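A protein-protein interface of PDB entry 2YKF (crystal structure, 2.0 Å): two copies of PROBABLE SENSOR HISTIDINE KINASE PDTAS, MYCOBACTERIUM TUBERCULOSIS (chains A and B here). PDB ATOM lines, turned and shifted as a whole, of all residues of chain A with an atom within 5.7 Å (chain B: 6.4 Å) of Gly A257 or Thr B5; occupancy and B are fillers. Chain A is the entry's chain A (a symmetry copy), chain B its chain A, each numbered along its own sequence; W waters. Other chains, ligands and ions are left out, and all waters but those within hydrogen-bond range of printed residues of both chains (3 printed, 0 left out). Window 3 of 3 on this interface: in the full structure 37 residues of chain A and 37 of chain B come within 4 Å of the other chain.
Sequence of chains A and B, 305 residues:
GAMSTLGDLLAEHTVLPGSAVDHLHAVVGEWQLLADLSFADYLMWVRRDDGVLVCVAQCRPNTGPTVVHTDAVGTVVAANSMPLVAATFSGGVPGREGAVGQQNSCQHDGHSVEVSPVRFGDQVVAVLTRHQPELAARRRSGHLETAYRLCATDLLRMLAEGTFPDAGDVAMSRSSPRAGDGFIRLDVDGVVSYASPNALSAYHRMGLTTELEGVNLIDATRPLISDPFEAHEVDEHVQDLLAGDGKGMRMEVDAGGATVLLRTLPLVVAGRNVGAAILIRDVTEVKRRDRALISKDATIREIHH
The side-chain hydroxyl of Thr B5 sits at hydrogen-bond distance from the side-chain carboxylate of Asp B8 (3.1 Å).
OG of Ser B4 sits at hydrogen-bond distance from NH1 of Arg A205.
No position is printed for both chains. Of the 5 pairs that touch across the chains among the printed residues, none has its exchanged pair printed and touching as well.
Of the 10 printed residues of chain B, 4 touch a printed residue of chain A. Printed residues of chain B that touch a printed residue of chain A: Ser B4, Thr B5, Leu B6 and Val B73. Hydrophobic or aromatic side chains of chain B that line the printed part of chain A: Leu B6 and Val B73. Of the 9 printed residues of chain A, 4 touch a printed residue of chain B. Among the printed residues, 5 pairs touch across the chains. Among the printed residues, no Asp or Glu carboxylate lies within 4 Å of a Lys or Arg side-chain nitrogen of the other chain.
Among the printed residues, merely in contact across the chains: Arg A205 with Val B73, Gly A257 with Thr B5, Ala A258 with Thr B5 and Glu A285 with Leu B6.
Gly A257 touches just one residue of chain B: Thr B5 (3.7 Å). Thr B5 touches just these residues of chain A: Gly A257 and Ala A258. Of the printed residues of chain B, Ala A258 touches Thr B5. Of the printed residues of chain A, Leu B6 touches Glu A285. Leu B9 touches none of the printed residues of chain A. Val B56 touches none of the printed residues of chain A.
Water W3 bridges OE2 of Glu A285 (2.7 Å) and N of Leu B6 (3.0 Å). Water W1 bridges O of Val B73 (2.8 Å) and NH1 of Arg A205 (2.9 Å). Water W2 bridges the side-chain carboxylate of Glu A285 and the backbone NH of Gly B7.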
ATOM      1  N   ARG A 205     -16.024 -11.936  15.362  1.00  0.00           N
ATOM      2  CA  ARG A 205     -16.860 -12.990  14.779  1.00  0.00           C
ATOM      3  C   ARG A 205     -18.232 -12.899  15.411  1.00  0.00           C
ATOM      4  O   ARG A 205     -19.228 -13.218  14.755  1.00  0.00           O
ATOM      5  CB  ARG A 205     -16.268 -14.400  15.064  1.00  0.00           C
ATOM      6  CG  ARG A 205     -14.931 -14.699  14.336  1.00  0.00           C
ATOM      7  CD  ARG A 205     -15.093 -14.262  12.751  1.00  0.00           C
ATOM      8  NE  ARG A 205     -13.868 -13.611  12.671  1.00  0.00           N
ATOM      9  CZ  ARG A 205     -13.545 -12.362  12.546  1.00  0.00           C
ATOM     10  NH1 ARG A 205     -14.217 -11.375  11.899  1.00  0.00           N
ATOM     11  NH2 ARG A 205     -12.330 -12.247  12.848  1.00  0.00           N
ATOM     12  N   SER A 226     -27.129 -13.894  21.356  1.00  0.00           N
ATOM     13  CA  SER A 226     -28.344 -14.200  20.547  1.00  0.00           C
ATOM     14  C   SER A 226     -29.583 -14.454  21.406  1.00  0.00           C
ATOM     15  O   SER A 226     -30.658 -13.923  21.116  1.00  0.00           O
ATOM     16  CB  SER A 226     -28.118 -15.411  19.618  1.00  0.00           C
ATOM     17  OG  SER A 226     -27.048 -15.155  18.681  1.00  0.00           O
ATOM     18  N   ALA A 255     -23.548 -15.983  19.666  1.00  0.00           N
ATOM     19  CA  ALA A 255     -23.622 -14.587  19.378  1.00  0.00           C
ATOM     20  C   ALA A 255     -23.302 -14.375  17.923  1.00  0.00           C
ATOM     21  O   ALA A 255     -22.175 -14.700  17.453  1.00  0.00           O
ATOM     22  CB  ALA A 255     -22.612 -13.822  20.210  1.00  0.00           C
ATOM     23  N   GLY A 256     -24.233 -13.777  17.192  1.00  0.00           N
ATOM     24  CA  GLY A 256     -23.871 -13.290  15.842  1.00  0.00           C
ATOM     25  C   GLY A 256     -23.469 -14.363  14.849  1.00  0.00           C
ATOM     26  O   GLY A 256     -22.617 -14.112  13.953  1.00  0.00           O
ATOM     27  N   GLY A 257     -24.060 -15.557  14.975  1.00  0.00           N
ATOM     28  CA  GLY A 257     -23.642 -16.684  14.122  1.00  0.00           C
ATOM     29  C   GLY A 257     -22.440 -17.473  14.676  1.00  0.00           C
ATOM     30  O   GLY A 257     -22.236 -18.574  14.258  1.00  0.00           O
ATOM     31  N   ALA A 258     -21.673 -16.886  15.624  1.00  0.00           N
ATOM     32  CA  ALA A 258     -20.499 -17.521  16.257  1.00  0.00           C
ATOM     33  C   ALA A 258     -20.889 -18.184  17.590  1.00  0.00           C
ATOM     34  O   ALA A 258     -21.952 -17.906  18.111  1.00  0.00           O
ATOM     35  CB  ALA A 258     -19.433 -16.447  16.522  1.00  0.00           C
ATOM     36  N   THR A 259     -20.070 -19.099  18.100  1.00  0.00           N
ATOM     37  CA  THR A 259     -20.274 -19.713  19.412  1.00  0.00           C
ATOM     38  C   THR A 259     -18.937 -19.569  20.105  1.00  0.00           C
ATOM     39  O   THR A 259     -17.892 -19.949  19.533  1.00  0.00           O
ATOM     40  CB  THR A 259     -20.600 -21.210  19.326  1.00  0.00           C
ATOM     41  OG1 THR A 259     -21.802 -21.366  18.566  1.00  0.00           O
ATOM     42  CG2 THR A 259     -20.816 -21.855  20.794  1.00  0.00           C
ATOM     43  N   THR A 284     -16.849 -21.835  17.055  1.00  0.00           N
ATOM     44  CA  THR A 284     -17.823 -21.899  15.960  1.00  0.00           C
ATOM     45  C   THR A 284     -17.622 -23.136  15.072  1.00  0.00           C
ATOM     46  O   THR A 284     -18.589 -23.865  14.819  1.00  0.00           O
ATOM     47  CB  THR A 284     -17.720 -20.627  15.115  1.00  0.00           C
ATOM     48  OG1 THR A 284     -17.909 -19.493  15.977  1.00  0.00           O
ATOM     49  CG2 THR A 284     -18.824 -20.580  13.991  1.00  0.00           C
ATOM     50  N   GLU A 285     -16.374 -23.375  14.650  1.00  0.00           N
ATOM     51  CA  GLU A 285     -16.051 -24.474  13.746  1.00  0.00           C
ATOM     52  C   GLU A 285     -15.617 -25.699  14.517  1.00  0.00           C
ATOM     53  O   GLU A 285     -15.508 -26.750  13.954  1.00  0.00           O
ATOM     54  CB  GLU A 285     -14.947 -24.079  12.759  1.00  0.00           C
ATOM     55  CG  GLU A 285     -15.120 -22.627  12.179  1.00  0.00           C
ATOM     56  CD  GLU A 285     -16.402 -22.479  11.391  1.00  0.00           C
ATOM     57  OE1 GLU A 285     -16.894 -23.531  10.923  1.00  0.00           O
ATOM     58  OE2 GLU A 285     -16.937 -21.360  11.271  1.00  0.00           O
ATOM     59  N   MET B   3     -21.860  -9.864  10.120  1.00  0.00           N
ATOM     60  CA  MET B   3     -21.860 -11.069   9.236  1.00  0.00           C
ATOM     61  C   MET B   3     -20.430 -11.642   9.065  1.00  0.00           C
ATOM     62  O   MET B   3     -19.820 -11.538   7.988  1.00  0.00           O
ATOM     63  CB  MET B   3     -22.427 -10.673   7.875  1.00  0.00           C
ATOM     64  CG  MET B   3     -21.822  -9.362   7.324  1.00  0.00           C
ATOM     65  SD  MET B   3     -21.534  -9.389   5.520  1.00  0.00           S
ATOM     66  CE  MET B   3     -20.650 -10.956   5.280  1.00  0.00           C
ATOM     67  N   SER B   4     -19.880 -12.235  10.121  1.00  0.00           N
ATOM     68  CA  SER B   4     -18.425 -12.386  10.138  1.00  0.00           C
ATOM     69  C   SER B   4     -17.868 -13.823  10.149  1.00  0.00           C
ATOM     70  O   SER B   4     -16.652 -14.047  10.078  1.00  0.00           O
ATOM     71  CB  SER B   4     -17.815 -11.545  11.269  1.00  0.00           C
ATOM     72  OG  SER B   4     -16.603 -10.936  10.827  1.00  0.00           O
ATOM     73  N   THR B   5     -18.749 -14.794  10.158  1.00  0.00           N
ATOM     74  CA  THR B   5     -18.306 -16.154  10.268  1.00  0.00           C
ATOM     75  C   THR B   5     -17.797 -16.660   8.900  1.00  0.00           C
ATOM     76  O   THR B   5     -18.163 -16.118   7.847  1.00  0.00           O
ATOM     77  CB  THR B   5     -19.440 -17.064  10.805  1.00  0.00           C
ATOM     78  OG1 THR B   5     -20.510 -17.074   9.860  1.00  0.00           O
ATOM     79  CG2 THR B   5     -19.936 -16.571  12.155  1.00  0.00           C
ATOM     80  N   LEU B   6     -16.965 -17.703   8.935  1.00  0.00           N
ATOM     81  CA  LEU B   6     -16.591 -18.442   7.730  1.00  0.00           C
ATOM     82  C   LEU B   6     -17.843 -18.774   6.865  1.00  0.00           C
ATOM     83  O   LEU B   6     -17.870 -18.486   5.658  1.00  0.00           O
ATOM     84  CB  LEU B   6     -15.864 -19.716   8.147  1.00  0.00           C
ATOM     85  CG  LEU B   6     -15.546 -20.739   7.039  1.00  0.00           C
ATOM     86  CD1 LEU B   6     -14.525 -20.168   6.071  1.00  0.00           C
ATOM     87  CD2 LEU B   6     -15.033 -22.076   7.640  1.00  0.00           C
ATOM     88  N   GLY B   7     -18.865 -19.392   7.462  1.00  0.00           N
ATOM     89  CA  GLY B   7     -20.107 -19.722   6.706  1.00  0.00           C
ATOM     90  C   GLY B   7     -20.732 -18.532   5.947  1.00  0.00           C
ATOM     91  O   GLY B   7     -20.999 -18.614   4.724  1.00  0.00           O
ATOM     92  N   ASP B   8     -20.947 -17.422   6.661  1.00  0.00           N
ATOM     93  CA  ASP B   8     -21.524 -16.187   6.051  1.00  0.00           C
ATOM     94  C   ASP B   8     -20.634 -15.673   4.939  1.00  0.00           C
ATOM     95  O   ASP B   8     -21.138 -15.341   3.851  1.00  0.00           O
ATOM     96  CB  ASP B   8     -21.868 -15.079   7.085  1.00  0.00           C
ATOM     97  CG  ASP B   8     -22.838 -15.569   8.180  1.00  0.00           C
ATOM     98  OD1 ASP B   8     -23.640 -16.518   7.908  1.00  0.00           O
ATOM     99  OD2 ASP B   8     -22.777 -15.027   9.320  1.00  0.00           O
ATOM    100  N   LEU B   9     -19.316 -15.661   5.169  1.00  0.00           N
ATOM    101  CA  LEU B   9     -18.369 -15.245   4.142  1.00  0.00           C
ATOM    102  C   LEU B   9     -18.341 -16.106   2.901  1.00  0.00           C
ATOM    103  O   LEU B   9     -18.300 -15.576   1.788  1.00  0.00           O
ATOM    104  CB  LEU B   9     -16.954 -15.111   4.704  1.00  0.00           C
ATOM    105  CG  LEU B   9     -16.805 -13.943   5.702  1.00  0.00           C
ATOM    106  CD1 LEU B   9     -15.352 -13.804   6.171  1.00  0.00           C
ATOM    107  CD2 LEU B   9     -17.360 -12.593   5.173  1.00  0.00           C
ATOM    108  N   LEU B  10     -18.348 -17.438   3.068  1.00  0.00           N
ATOM    109  CA  LEU B  10     -18.348 -18.327   1.899  1.00  0.00           C
ATOM    110  C   LEU B  10     -19.682 -18.205   1.079  1.00  0.00           C
ATOM    111  O   LEU B  10     -19.667 -18.302  -0.129  1.00  0.00           O
ATOM    112  CB  LEU B  10     -18.069 -19.797   2.320  1.00  0.00           C
ATOM    113  CG  LEU B  10     -16.726 -20.126   2.989  1.00  0.00           C
ATOM    114  CD1 LEU B  10     -16.692 -21.619   3.442  1.00  0.00           C
ATOM    115  CD2 LEU B  10     -15.641 -19.854   2.055  1.00  0.00           C
ATOM    116  N   VAL B  56     -11.114 -15.447   4.709  1.00  0.00           N
ATOM    117  CA  VAL B  56     -12.351 -15.893   5.320  1.00  0.00           C
ATOM    118  C   VAL B  56     -12.088 -16.525   6.718  1.00  0.00           C
ATOM    119  O   VAL B  56     -13.048 -16.810   7.408  1.00  0.00           O
ATOM    120  CB  VAL B  56     -13.129 -16.941   4.450  1.00  0.00           C
ATOM    121  CG1 VAL B  56     -13.653 -16.304   3.100  1.00  0.00           C
ATOM    122  CG2 VAL B  56     -12.211 -18.103   4.129  1.00  0.00           C
ATOM    123  N   VAL B  73      -9.803 -11.264   8.875  1.00  0.00           N
ATOM    124  CA  VAL B  73     -10.978 -11.903   8.358  1.00  0.00           C
ATOM    125  C   VAL B  73     -11.895 -10.855   7.731  1.00  0.00           C
ATOM    126  O   VAL B  73     -12.091  -9.782   8.322  1.00  0.00           O
ATOM    127  CB  VAL B  73     -11.745 -12.638   9.454  1.00  0.00           C
ATOM    128  CG1 VAL B  73     -12.975 -13.238   8.862  1.00  0.00           C
ATOM    129  CG2 VAL B  73     -10.836 -13.790  10.065  1.00  0.00           C
HETATM  130  O   HOH W   1     -12.843  -8.970  10.910  1.00  0.00           O
HETATM  131  O   HOH W   2     -19.371 -20.445  10.166  1.00  0.00           O
HETATM  132  O   HOH W   3     -15.995 -18.831  11.575  1.00  0.00           O
